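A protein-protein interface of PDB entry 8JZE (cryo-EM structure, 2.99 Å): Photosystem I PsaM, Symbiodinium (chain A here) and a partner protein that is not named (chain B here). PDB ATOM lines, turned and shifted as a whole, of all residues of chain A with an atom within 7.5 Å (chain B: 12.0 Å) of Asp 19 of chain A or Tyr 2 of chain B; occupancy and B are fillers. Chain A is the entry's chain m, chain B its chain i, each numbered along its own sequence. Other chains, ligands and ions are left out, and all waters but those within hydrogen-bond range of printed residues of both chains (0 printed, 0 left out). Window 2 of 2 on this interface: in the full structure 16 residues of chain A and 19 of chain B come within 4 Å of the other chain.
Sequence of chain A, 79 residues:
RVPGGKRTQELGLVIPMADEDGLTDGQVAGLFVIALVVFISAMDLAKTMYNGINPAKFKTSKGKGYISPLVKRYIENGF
Asp 19 of chain A touches just these residues of chain B: Lys 1 (3.6 Å) and Tyr 2 (3.6 Å). Tyr 2 of chain B touches three residues of chain A. Ala 18 of chain A touches one residue of chain B. Of chain B, only Lys 1 (3.4 Å) and Tyr 2 (3.2 Å) come within 4 Å of Glu 20 of chain A. Printed residues of chain A within 4 Å of Gln 5 of chain B: Asp 21. Printed residues of chain A within 4 Å of Lys 1 of chain B: Asp 19 (3.6 Å), Glu 20 (3.4 Å) and Asp 21 (3.5 Å). Of the printed residues of chain A, Asp 4 of chain B touches Asp 21.
Ala 18 of chain A touches Tyr 2 of chain B. O of Asp 19 of chain A touches C of Lys 1 of chain B, at 3.6 Å. Tyr 2 of chain B touches Asp 19 of chain A (N to O, 3.6 Å). Glu 20 of chain A touches Tyr 2 of chain B. Asp 21 of chain A touches Lys 1 of chain B (OD1 to O, 3.5 Å). Asp 21 of chain A touches Asp 4 of chain B.
NE2 of Gln 5 of chain B lies within hydrogen-bond range of OD1 of Asp 21 of chain A (2.9 Å). O of Lys 1 of chain B sits close to O of Glu 20 of chain A (3.4 Å). OD1 of Asp 21 of chain A lies close to O of Gly 3 of chain B (2.8 Å).
The backbone NH (N) of Lys 1 of chain B lies within hydrogen-bond range of the side-chain carboxylate (OD2) of Asp 4 of chain B. The backbone carbonyl oxygen of Tyr 2 of chain B lies close to the side-chain amide oxygen of Gln 5 of chain B (3.3 Å). O of Gly 3 of chain B lies close to OE1 of Gln 5 of chain B (3.2 Å).
Of the 9 printed residues of chain B, 5 touch a printed residue of chain A. Along chain B the printed residues that touch a printed residue of chain A span positions 1 to 5. Of the 7 printed residues of chain A, 4 touch a printed residue of chain B. Printed residues of chain A that touch a printed residue of chain B: Ala 18, Asp 19, Glu 20 and Asp 21. Among the printed residues, no Asp or Glu carboxylate lies within 4 Å of a Lys or Arg side-chain nitrogen of the other chain.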
ATOM      1  N   PRO A  16      -7.492  16.193 -15.734  1.00  0.00           N
ATOM      2  CA  PRO A  16      -8.136  17.413 -15.240  1.00  0.00           C
ATOM      3  C   PRO A  16      -9.069  17.110 -14.082  1.00  0.00           C
ATOM      4  O   PRO A  16      -9.684  16.044 -14.010  1.00  0.00           O
ATOM      5  CB  PRO A  16      -8.917  17.923 -16.459  1.00  0.00           C
ATOM      6  CG  PRO A  16      -8.335  17.202 -17.635  1.00  0.00           C
ATOM      7  CD  PRO A  16      -7.889  15.878 -17.113  1.00  0.00           C
ATOM      8  N   MET A  17      -9.165  18.067 -13.165  1.00  0.00           N
ATOM      9  CA  MET A  17     -10.080  17.974 -12.038  1.00  0.00           C
ATOM     10  C   MET A  17     -10.966  19.208 -12.018  1.00  0.00           C
ATOM     11  O   MET A  17     -10.464  20.335 -12.081  1.00  0.00           O
ATOM     12  CB  MET A  17      -9.333  17.856 -10.711  1.00  0.00           C
ATOM     13  CG  MET A  17      -8.447  16.639 -10.595  1.00  0.00           C
ATOM     14  SD  MET A  17      -7.453  16.747  -9.101  1.00  0.00           S
ATOM     15  CE  MET A  17      -6.994  18.475  -9.181  1.00  0.00           C
ATOM     16  N   ALA A  18     -12.274  18.992 -11.925  1.00  0.00           N
ATOM     17  CA  ALA A  18     -13.201  20.108 -11.825  1.00  0.00           C
ATOM     18  C   ALA A  18     -12.954  20.886 -10.541  1.00  0.00           C
ATOM     19  O   ALA A  18     -12.788  20.306  -9.465  1.00  0.00           O
ATOM     20  CB  ALA A  18     -14.643  19.604 -11.868  1.00  0.00           C
ATOM     21  N   ASP A  19     -12.920  22.212 -10.659  1.00  0.00           N
ATOM     22  CA  ASP A  19     -12.805  23.061  -9.481  1.00  0.00           C
ATOM     23  C   ASP A  19     -14.127  23.219  -8.743  1.00  0.00           C
ATOM     24  O   ASP A  19     -14.124  23.666  -7.592  1.00  0.00           O
ATOM     25  CB  ASP A  19     -12.262  24.438  -9.872  1.00  0.00           C
ATOM     26  CG  ASP A  19     -12.925  24.997 -11.114  1.00  0.00           C
ATOM     27  OD1 ASP A  19     -13.695  24.260 -11.761  1.00  0.00           O
ATOM     28  OD2 ASP A  19     -12.675  26.176 -11.445  1.00  0.00           O
ATOM     29  N   GLU A  20     -15.245  22.859  -9.369  1.00  0.00           N
ATOM     30  CA  GLU A  20     -16.541  22.891  -8.705  1.00  0.00           C
ATOM     31  C   GLU A  20     -16.714  21.615  -7.883  1.00  0.00           C
ATOM     32  O   GLU A  20     -15.775  20.840  -7.686  1.00  0.00           O
ATOM     33  CB  GLU A  20     -17.662  23.081  -9.724  1.00  0.00           C
ATOM     34  CG  GLU A  20     -17.816  21.947 -10.727  1.00  0.00           C
ATOM     35  CD  GLU A  20     -17.187  22.264 -12.069  1.00  0.00           C
ATOM     36  OE1 GLU A  20     -16.089  22.855 -12.088  1.00  0.00           O
ATOM     37  OE2 GLU A  20     -17.797  21.931 -13.108  1.00  0.00           O
ATOM     38  N   ASP A  21     -17.930  21.380  -7.395  1.00  0.00           N
ATOM     39  CA  ASP A  21     -18.176  20.277  -6.476  1.00  0.00           C
ATOM     40  C   ASP A  21     -18.636  19.005  -7.172  1.00  0.00           C
ATOM     41  O   ASP A  21     -18.419  17.909  -6.642  1.00  0.00           O
ATOM     42  CB  ASP A  21     -19.222  20.686  -5.434  1.00  0.00           C
ATOM     43  CG  ASP A  21     -19.184  19.814  -4.195  1.00  0.00           C
ATOM     44  OD1 ASP A  21     -18.203  19.061  -4.030  1.00  0.00           O
ATOM     45  OD2 ASP A  21     -20.134  19.880  -3.389  1.00  0.00           O
ATOM     46  N   GLY A  22     -19.246  19.112  -8.346  1.00  0.00           N
ATOM     47  CA  GLY A  22     -19.895  17.961  -8.939  1.00  0.00           C
ATOM     48  C   GLY A  22     -21.371  17.938  -8.605  1.00  0.00           C
ATOM     49  O   GLY A  22     -22.173  18.595  -9.275  1.00  0.00           O
ATOM     50  N   LYS B   1     -15.416  23.885  -3.652  1.00  0.00           N
ATOM     51  CA  LYS B   1     -14.148  23.236  -3.966  1.00  0.00           C
ATOM     52  C   LYS B   1     -14.392  21.814  -4.470  1.00  0.00           C
ATOM     53  O   LYS B   1     -15.477  21.266  -4.278  1.00  0.00           O
ATOM     54  CB  LYS B   1     -13.235  23.222  -2.736  1.00  0.00           C
ATOM     55  CG  LYS B   1     -11.766  23.007  -3.057  1.00  0.00           C
ATOM     56  CD  LYS B   1     -11.250  24.088  -3.989  1.00  0.00           C
ATOM     57  CE  LYS B   1      -9.893  23.720  -4.563  1.00  0.00           C
ATOM     58  NZ  LYS B   1      -8.890  23.436  -3.499  1.00  0.00           N
ATOM     59  N   TYR B   2     -13.385  21.221  -5.118  1.00  0.00           N
ATOM     60  CA  TYR B   2     -13.522  19.850  -5.600  1.00  0.00           C
ATOM     61  C   TYR B   2     -13.700  18.859  -4.461  1.00  0.00           C
ATOM     62  O   TYR B   2     -14.207  17.755  -4.687  1.00  0.00           O
ATOM     63  CB  TYR B   2     -12.317  19.446  -6.450  1.00  0.00           C
ATOM     64  CG  TYR B   2     -12.414  18.029  -6.969  1.00  0.00           C
ATOM     65  CD1 TYR B   2     -13.446  17.652  -7.818  1.00  0.00           C
ATOM     66  CD2 TYR B   2     -11.486  17.065  -6.597  1.00  0.00           C
ATOM     67  CE1 TYR B   2     -13.548  16.360  -8.288  1.00  0.00           C
ATOM     68  CE2 TYR B   2     -11.580  15.769  -7.065  1.00  0.00           C
ATOM     69  CZ  TYR B   2     -12.612  15.423  -7.909  1.00  0.00           C
ATOM     70  OH  TYR B   2     -12.710  14.133  -8.378  1.00  0.00           O
ATOM     71  N   GLY B   3     -13.311  19.228  -3.246  1.00  0.00           N
ATOM     72  CA  GLY B   3     -13.583  18.385  -2.102  1.00  0.00           C
ATOM     73  C   GLY B   3     -15.029  18.515  -1.680  1.00  0.00           C
ATOM     74  O   GLY B   3     -15.926  18.536  -2.529  1.00  0.00           O
ATOM     75  N   ASP B   4     -15.269  18.548  -0.370  1.00  0.00           N
ATOM     76  CA  ASP B   4     -16.585  18.807   0.208  1.00  0.00           C
ATOM     77  C   ASP B   4     -17.527  17.628  -0.010  1.00  0.00           C
ATOM     78  O   ASP B   4     -18.635  17.605   0.534  1.00  0.00           O
ATOM     79  CB  ASP B   4     -17.188  20.097  -0.361  1.00  0.00           C
ATOM     80  CG  ASP B   4     -16.206  21.255  -0.354  1.00  0.00           C
ATOM     81  OD1 ASP B   4     -15.209  21.185   0.396  1.00  0.00           O
ATOM     82  OD2 ASP B   4     -16.430  22.234  -1.098  1.00  0.00           O
ATOM     83  N   GLN B   5     -17.097  16.642  -0.798  1.00  0.00           N
ATOM     84  CA  GLN B   5     -17.736  15.335  -0.809  1.00  0.00           C
ATOM     85  C   GLN B   5     -17.094  14.387   0.187  1.00  0.00           C
ATOM     86  O   GLN B   5     -17.686  13.353   0.517  1.00  0.00           O
ATOM     87  CB  GLN B   5     -17.681  14.710  -2.208  1.00  0.00           C
ATOM     88  CG  GLN B   5     -18.818  15.121  -3.128  1.00  0.00           C
ATOM     89  CD  GLN B   5     -18.370  16.049  -4.237  1.00  0.00           C
ATOM     90  OE1 GLN B   5     -17.175  16.261  -4.443  1.00  0.00           O
ATOM     91  NE2 GLN B   5     -19.331  16.611  -4.960  1.00  0.00           N
ATOM     92  N   ARG B   6     -15.895  14.723   0.665  1.00  0.00           N
ATOM     93  CA  ARG B   6     -15.237  13.939   1.699  1.00  0.00           C
ATOM     94  C   ARG B   6     -15.965  14.026   3.031  1.00  0.00           C
ATOM     95  O   ARG B   6     -15.706  13.207   3.917  1.00  0.00           O
ATOM     96  CB  ARG B   6     -13.785  14.396   1.849  1.00  0.00           C
ATOM     97  CG  ARG B   6     -12.959  14.228   0.580  1.00  0.00           C
ATOM     98  CD  ARG B   6     -11.606  14.921   0.681  1.00  0.00           C
ATOM     99  NE  ARG B   6     -11.738  16.371   0.762  1.00  0.00           N
ATOM    100  CZ  ARG B   6     -10.720  17.221   0.751  1.00  0.00           C
ATOM    101  NH1 ARG B   6      -9.470  16.799   0.656  1.00  0.00           N
ATOM    102  NH2 ARG B   6     -10.962  18.525   0.836  1.00  0.00           N
ATOM    103  N   LYS B   7     -16.867  14.999   3.193  1.00  0.00           N
ATOM    104  CA  LYS B   7     -17.720  15.013   4.376  1.00  0.00           C
ATOM    105  C   LYS B   7     -18.620  13.785   4.404  1.00  0.00           C
ATOM    106  O   LYS B   7     -18.912  13.243   5.475  1.00  0.00           O
ATOM    107  CB  LYS B   7     -18.553  16.300   4.420  1.00  0.00           C
ATOM    108  CG  LYS B   7     -19.659  16.389   3.375  1.00  0.00           C
ATOM    109  CD  LYS B   7     -20.654  17.500   3.689  1.00  0.00           C
ATOM    110  CE  LYS B   7     -20.144  18.861   3.246  1.00  0.00           C
ATOM    111  NZ  LYS B   7     -20.063  18.962   1.763  1.00  0.00           N
ATOM    112  N   PHE B   8     -19.068  13.331   3.231  1.00  0.00           N
ATOM    113  CA  PHE B   8     -19.822  12.087   3.156  1.00  0.00           C
ATOM    114  C   PHE B   8     -18.910  10.881   3.348  1.00  0.00           C
ATOM    115  O   PHE B   8     -19.298   9.903   3.996  1.00  0.00           O
ATOM    116  CB  PHE B   8     -20.555  11.994   1.818  1.00  0.00           C
ATOM    117  CG  PHE B   8     -21.845  12.768   1.772  1.00  0.00           C
ATOM    118  CD1 PHE B   8     -21.859  14.103   1.402  1.00  0.00           C
ATOM    119  CD2 PHE B   8     -23.045  12.152   2.089  1.00  0.00           C
ATOM    120  CE1 PHE B   8     -23.048  14.812   1.355  1.00  0.00           C
ATOM    121  CE2 PHE B   8     -24.235  12.854   2.044  1.00  0.00           C
ATOM    122  CZ  PHE B   8     -24.236  14.185   1.677  1.00  0.00           C
ATOM    123  N   ALA B   9     -17.700  10.936   2.783  1.00  0.00           N
ATOM    124  CA  ALA B   9     -16.789   9.798   2.855  1.00  0.00           C
ATOM    125  C   ALA B   9     -16.361   9.516   4.287  1.00  0.00           C
ATOM    126  O   ALA B   9     -16.345   8.357   4.716  1.00  0.00           O
ATOM    127  CB  ALA B   9     -15.568  10.047   1.970  1.00  0.00           C
